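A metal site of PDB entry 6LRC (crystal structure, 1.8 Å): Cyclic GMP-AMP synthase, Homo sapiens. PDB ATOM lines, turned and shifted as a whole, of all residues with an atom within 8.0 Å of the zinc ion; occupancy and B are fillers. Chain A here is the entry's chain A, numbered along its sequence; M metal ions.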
ATOM      1  N   LEU A 231      12.136  16.093 -19.359  1.00  0.00           N
ATOM      2  CA  LEU A 231      13.492  16.564 -19.057  1.00  0.00           C
ATOM      3  C   LEU A 231      14.351  15.468 -18.453  1.00  0.00           C
ATOM      4  O   LEU A 231      15.549  15.369 -18.768  1.00  0.00           O
ATOM      5  CB  LEU A 231      13.439  17.763 -18.103  1.00  0.00           C
ATOM      6  CG  LEU A 231      13.153  19.128 -18.740  1.00  0.00           C
ATOM      7  CD1 LEU A 231      13.055  20.224 -17.681  1.00  0.00           C
ATOM      8  CD2 LEU A 231      14.230  19.451 -19.766  1.00  0.00           C
ATOM      9  N   ASN A 232      13.777  14.646 -17.573  1.00  0.00           N
ATOM     10  CA  ASN A 232      14.517  13.573 -16.919  1.00  0.00           C
ATOM     11  C   ASN A 232      14.624  12.318 -17.776  1.00  0.00           C
ATOM     12  O   ASN A 232      15.327  11.375 -17.387  1.00  0.00           O
ATOM     13  CB  ASN A 232      13.861  13.230 -15.609  1.00  0.00           C
ATOM     14  CG  ASN A 232      14.054  14.326 -14.589  1.00  0.00           C
ATOM     15  OD1 ASN A 232      14.892  15.205 -14.791  1.00  0.00           O
ATOM     16  ND2 ASN A 232      13.283  14.286 -13.499  1.00  0.00           N
ATOM     17  N   ASN A 233      13.935  12.273 -18.898  1.00  0.00           N
ATOM     18  CA  ASN A 233      13.973  11.130 -19.795  1.00  0.00           C
ATOM     19  C   ASN A 233      13.951  11.695 -21.215  1.00  0.00           C
ATOM     20  O   ASN A 233      12.968  11.581 -21.949  1.00  0.00           O
ATOM     21  CB  ASN A 233      12.806  10.183 -19.523  1.00  0.00           C
ATOM     22  CG  ASN A 233      12.983   8.840 -20.183  1.00  0.00           C
ATOM     23  OD1 ASN A 233      13.994   8.584 -20.846  1.00  0.00           O
ATOM     24  ND2 ASN A 233      12.005   7.972 -20.005  1.00  0.00           N
ATOM     25  N   HIS A 234      15.072  12.285 -21.628  1.00  0.00           N
ATOM     26  CA  HIS A 234      15.092  13.293 -22.682  1.00  0.00           C
ATOM     27  C   HIS A 234      15.721  12.832 -23.987  1.00  0.00           C
ATOM     28  O   HIS A 234      15.803  13.634 -24.928  1.00  0.00           O
ATOM     29  CB  HIS A 234      15.891  14.508 -22.172  1.00  0.00           C
ATOM     30  CG  HIS A 234      17.289  14.145 -21.771  1.00  0.00           C
ATOM     31  ND1 HIS A 234      17.756  14.279 -20.480  1.00  0.00           N
ATOM     32  CD2 HIS A 234      18.319  13.627 -22.483  1.00  0.00           C
ATOM     33  CE1 HIS A 234      19.014  13.893 -20.427  1.00  0.00           C
ATOM     34  NE2 HIS A 234      19.376  13.477 -21.634  1.00  0.00           N
ATOM     35  N   GLY A 235      16.229  11.612 -24.072  1.00  0.00           N
ATOM     36  CA  GLY A 235      16.957  11.181 -25.250  1.00  0.00           C
ATOM     37  C   GLY A 235      16.075  10.348 -26.173  1.00  0.00           C
ATOM     38  O   GLY A 235      15.057   9.771 -25.763  1.00  0.00           O
ATOM     39  N   LYS A 236      16.449  10.331 -27.462  1.00  0.00           N
ATOM     40  CA  LYS A 236      15.887   9.320 -28.355  1.00  0.00           C
ATOM     41  C   LYS A 236      16.264   7.935 -27.859  1.00  0.00           C
ATOM     42  O   LYS A 236      15.435   7.023 -27.814  1.00  0.00           O
ATOM     43  CB  LYS A 236      16.381   9.520 -29.791  1.00  0.00           C
ATOM     44  CG  LYS A 236      15.786   8.474 -30.773  1.00  0.00           C
ATOM     45  CD  LYS A 236      15.894   8.889 -32.233  1.00  0.00           C
ATOM     46  CE  LYS A 236      14.957  10.029 -32.579  1.00  0.00           C
ATOM     47  NZ  LYS A 236      13.582   9.531 -32.612  1.00  0.00           N
ATOM     48  N   SER A 237      17.528   7.777 -27.473  1.00  0.00           N
ATOM     49  CA  SER A 237      17.982   6.539 -26.869  1.00  0.00           C
ATOM     50  C   SER A 237      17.506   6.475 -25.422  1.00  0.00           C
ATOM     51  O   SER A 237      17.638   7.448 -24.658  1.00  0.00           O
ATOM     52  CB  SER A 237      19.502   6.431 -26.934  1.00  0.00           C
ATOM     53  OG  SER A 237      19.975   5.323 -26.193  1.00  0.00           O
ATOM     54  N   THR A 239      19.033   4.938 -23.252  1.00  0.00           N
ATOM     55  CA  THR A 239      20.229   4.965 -22.427  1.00  0.00           C
ATOM     56  C   THR A 239      21.004   6.271 -22.583  1.00  0.00           C
ATOM     57  O   THR A 239      22.172   6.337 -22.211  1.00  0.00           O
ATOM     58  CB  THR A 239      21.141   3.766 -22.721  1.00  0.00           C
ATOM     59  OG1 THR A 239      21.235   3.530 -24.139  1.00  0.00           O
ATOM     60  CG2 THR A 239      20.619   2.506 -22.045  1.00  0.00           C
ATOM     61  N   CYS A 240      20.367   7.308 -23.148  1.00  0.00           N
ATOM     62  CA  CYS A 240      20.993   8.625 -23.215  1.00  0.00           C
ATOM     63  C   CYS A 240      21.498   9.027 -21.836  1.00  0.00           C
ATOM     64  O   CYS A 240      20.786   8.886 -20.839  1.00  0.00           O
ATOM     65  CB  CYS A 240      19.991   9.669 -23.725  1.00  0.00           C
ATOM     66  SG  CYS A 240      20.767  11.281 -24.267  1.00  0.00           S
ATOM     67  N   CYS A 241      22.742   9.484 -21.788  1.00  0.00           N
ATOM     68  CA  CYS A 241      23.417   9.953 -20.578  1.00  0.00           C
ATOM     69  C   CYS A 241      23.640   8.858 -19.535  1.00  0.00           C
ATOM     70  O   CYS A 241      24.027   9.180 -18.409  1.00  0.00           O
ATOM     71  CB  CYS A 241      22.660  11.119 -19.932  1.00  0.00           C
ATOM     72  SG  CYS A 241      22.908  12.673 -20.844  1.00  0.00           S
ATOM     73  N   GLU A 242      23.439   7.580 -19.863  1.00  0.00           N
ATOM     74  CA  GLU A 242      23.684   6.526 -18.878  1.00  0.00           C
ATOM     75  C   GLU A 242      25.070   5.908 -19.024  1.00  0.00           C
ATOM     76  O   GLU A 242      25.443   5.048 -18.220  1.00  0.00           O
ATOM     77  CB  GLU A 242      22.611   5.432 -18.963  1.00  0.00           C
ATOM     78  CG  GLU A 242      21.269   5.916 -18.443  1.00  0.00           C
ATOM     79  CD  GLU A 242      20.337   4.756 -18.078  1.00  0.00           C
ATOM     80  OE1 GLU A 242      19.271   5.018 -17.493  1.00  0.00           O
ATOM     81  OE2 GLU A 242      20.694   3.585 -18.334  1.00  0.00           O
ATOM     82  N   ASN A 243      25.824   6.309 -20.042  1.00  0.00           N
ATOM     83  CA  ASN A 243      27.176   5.806 -20.242  1.00  0.00           C
ATOM     84  C   ASN A 243      27.967   6.884 -20.988  1.00  0.00           C
ATOM     85  O   ASN A 243      27.409   7.891 -21.437  1.00  0.00           O
ATOM     86  CB  ASN A 243      27.181   4.500 -21.044  1.00  0.00           C
ATOM     87  CG  ASN A 243      26.452   4.635 -22.360  1.00  0.00           C
ATOM     88  OD1 ASN A 243      26.933   5.294 -23.280  1.00  0.00           O
ATOM     89  ND2 ASN A 243      25.286   3.995 -22.473  1.00  0.00           N
ATOM     90  N   GLU A 246      27.120   7.899 -24.690  1.00  0.00           N
ATOM     91  CA  GLU A 246      25.848   8.577 -24.959  1.00  0.00           C
ATOM     92  C   GLU A 246      25.620   9.812 -24.087  1.00  0.00           C
ATOM     93  O   GLU A 246      24.476  10.242 -23.914  1.00  0.00           O
ATOM     94  CB  GLU A 246      24.683   7.603 -24.778  1.00  0.00           C
ATOM     95  CG  GLU A 246      24.790   6.338 -25.625  1.00  0.00           C
ATOM     96  CD  GLU A 246      23.529   5.506 -25.543  1.00  0.00           C
ATOM     97  OE1 GLU A 246      22.467   5.973 -26.017  1.00  0.00           O
ATOM     98  OE2 GLU A 246      23.578   4.394 -24.977  1.00  0.00           O
ATOM     99  N   LYS A 247      26.689  10.418 -23.560  1.00  0.00           N
ATOM    100  CA  LYS A 247      26.506  11.656 -22.817  1.00  0.00           C
ATOM    101  C   LYS A 247      26.100  12.780 -23.775  1.00  0.00           C
ATOM    102  O   LYS A 247      26.782  13.040 -24.769  1.00  0.00           O
ATOM    103  CB  LYS A 247      27.783  12.041 -22.072  1.00  0.00           C
ATOM    104  CG  LYS A 247      28.223  11.031 -21.013  1.00  0.00           C
ATOM    105  CD  LYS A 247      27.256  10.957 -19.843  1.00  0.00           C
ATOM    106  CE  LYS A 247      27.827  10.118 -18.702  1.00  0.00           C
ATOM    107  NZ  LYS A 247      26.883   9.997 -17.549  1.00  0.00           N
ATOM    108  N   CYS A 248      24.988  13.442 -23.468  1.00  0.00           N
ATOM    109  CA  CYS A 248      24.506  14.572 -24.249  1.00  0.00           C
ATOM    110  C   CYS A 248      24.536  15.843 -23.380  1.00  0.00           C
ATOM    111  O   CYS A 248      24.802  15.796 -22.185  1.00  0.00           O
ATOM    112  CB  CYS A 248      23.093  14.302 -24.805  1.00  0.00           C
ATOM    113  SG  CYS A 248      21.685  14.756 -23.753  1.00  0.00           S
ATOM    114  N   CYS A 249      24.296  17.004 -24.005  1.00  0.00           N
ATOM    115  CA  CYS A 249      24.313  18.282 -23.283  1.00  0.00           C
ATOM    116  C   CYS A 249      22.952  18.973 -23.285  1.00  0.00           C
ATOM    117  O   CYS A 249      22.889  20.177 -23.025  1.00  0.00           O
ATOM    118  CB  CYS A 249      25.371  19.227 -23.850  1.00  0.00           C
ATOM    119  SG  CYS A 249      25.145  19.697 -25.583  1.00  0.00           S
ATOM    120  N   ARG A 250      21.866  18.243 -23.491  1.00  0.00           N
ATOM    121  CA  ARG A 250      20.529  18.859 -23.437  1.00  0.00           C
ATOM    122  C   ARG A 250      20.310  19.569 -22.111  1.00  0.00           C
ATOM    123  O   ARG A 250      19.968  20.763 -22.078  1.00  0.00           O
ATOM    124  CB  ARG A 250      19.445  17.802 -23.669  1.00  0.00           C
ATOM    125  CG  ARG A 250      19.433  17.133 -25.065  1.00  0.00           C
ATOM    126  CD  ARG A 250      18.066  16.493 -25.269  1.00  0.00           C
ATOM    127  NE  ARG A 250      17.810  15.851 -26.552  1.00  0.00           N
ATOM    128  CZ  ARG A 250      18.322  14.682 -26.953  1.00  0.00           C
ATOM    129  NH1 ARG A 250      19.194  14.019 -26.210  1.00  0.00           N
ATOM    130  NH2 ARG A 250      17.960  14.175 -28.140  1.00  0.00           N
ATOM    131  N   LYS A 251      20.453  18.852 -21.001  1.00  0.00           N
ATOM    132  CA  LYS A 251      20.118  19.466 -19.718  1.00  0.00           C
ATOM    133  C   LYS A 251      21.039  20.631 -19.379  1.00  0.00           C
ATOM    134  O   LYS A 251      20.597  21.641 -18.804  1.00  0.00           O
ATOM    135  CB  LYS A 251      20.146  18.416 -18.614  1.00  0.00           C
ATOM    136  CG  LYS A 251      19.054  17.361 -18.793  1.00  0.00           C
ATOM    137  CD  LYS A 251      18.930  16.521 -17.525  1.00  0.00           C
ATOM    138  CE  LYS A 251      17.880  17.110 -16.594  1.00  0.00           C
ATOM    139  NZ  LYS A 251      17.017  16.048 -16.051  1.00  0.00           N
ATOM    140  N   ASP A 296      20.104  12.220 -30.757  1.00  0.00           N
ATOM    141  CA  ASP A 296      21.052  12.391 -29.666  1.00  0.00           C
ATOM    142  C   ASP A 296      22.405  12.862 -30.155  1.00  0.00           C
ATOM    143  O   ASP A 296      23.082  13.628 -29.454  1.00  0.00           O
ATOM    144  CB  ASP A 296      21.220  11.089 -28.884  1.00  0.00           C
ATOM    145  CG  ASP A 296      19.934  10.645 -28.209  1.00  0.00           C
ATOM    146  OD1 ASP A 296      19.032  11.486 -27.964  1.00  0.00           O
ATOM    147  OD2 ASP A 296      19.831   9.440 -27.901  1.00  0.00           O
ATOM    148  N   TRP A 299      23.432  16.432 -29.988  1.00  0.00           N
ATOM    149  CA  TRP A 299      23.634  17.010 -28.672  1.00  0.00           C
ATOM    150  C   TRP A 299      24.876  16.434 -27.997  1.00  0.00           C
ATOM    151  O   TRP A 299      24.940  16.368 -26.769  1.00  0.00           O
ATOM    152  CB  TRP A 299      22.415  16.774 -27.775  1.00  0.00           C
ATOM    153  CG  TRP A 299      21.143  17.451 -28.251  1.00  0.00           C
ATOM    154  CD1 TRP A 299      20.207  16.944 -29.131  1.00  0.00           C
ATOM    155  CD2 TRP A 299      20.672  18.729 -27.847  1.00  0.00           C
ATOM    156  NE1 TRP A 299      19.186  17.843 -29.302  1.00  0.00           N
ATOM    157  CE2 TRP A 299      19.438  18.945 -28.510  1.00  0.00           C
ATOM    158  CE3 TRP A 299      21.157  19.715 -26.983  1.00  0.00           C
ATOM    159  CZ2 TRP A 299      18.691  20.107 -28.361  1.00  0.00           C
ATOM    160  CZ3 TRP A 299      20.410  20.867 -26.825  1.00  0.00           C
ATOM    161  CH2 TRP A 299      19.193  21.060 -27.502  1.00  0.00           C
ATOM    162  N   ARG A 301      28.169  15.979 -26.139  1.00  0.00           N
ATOM    163  CA  ARG A 301      28.803  16.855 -25.150  1.00  0.00           C
ATOM    164  C   ARG A 301      30.061  17.541 -25.673  1.00  0.00           C
ATOM    165  O   ARG A 301      30.402  18.649 -25.241  1.00  0.00           O
ATOM    166  CB  ARG A 301      29.117  16.030 -23.890  1.00  0.00           C
ATOM    167  CG  ARG A 301      29.992  16.736 -22.864  1.00  0.00           C
ATOM    168  CD  ARG A 301      29.629  16.267 -21.470  1.00  0.00           C
ATOM    169  NE  ARG A 301      28.233  16.577 -21.166  1.00  0.00           N
ATOM    170  CZ  ARG A 301      27.814  17.729 -20.656  1.00  0.00           C
ATOM    171  NH1 ARG A 301      28.682  18.692 -20.358  1.00  0.00           N
ATOM    172  NH2 ARG A 301      26.522  17.904 -20.419  1.00  0.00           N
HETATM  173 ZN    ZN M   1      21.206  12.765 -22.571  1.00  0.00          ZN
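NE2 of His 234 is bound to the zinc ion (2.2 Å).
The zinc ion is bound by SG of Cys 240.
SG of Cys 248 binds the zinc ion (2.4 Å).
The zinc ion is bound by SG of Cys 241 (2.4 Å).
The zinc ion has four donor atoms within binding distance.
The guanidinium group of Arg 250 sits close to the backbone carbonyl oxygen of His 234, at 3.4 Å.
O of Leu 231 is in hydrogen-bond range of ND1 of His 234 (3.0 Å).
SG of Cys 240 lies close to NH1 of Arg 250.
The side-chain sulfur (SG) of Cys 248 sits close to the backbone NH (N) of Arg 250 (3.5 Å).
O of Cys 248 lies within hydrogen-bond range of NH2 of Arg 301 (3.2 Å).
N of Cys 241 is in hydrogen-bond range of O of Glu 246 (2.8 Å).
The side-chain amino group (NZ) of Lys 247 lies within hydrogen-bond range of the backbone carbonyl oxygen (O) of Cys 241 (3.1 Å).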
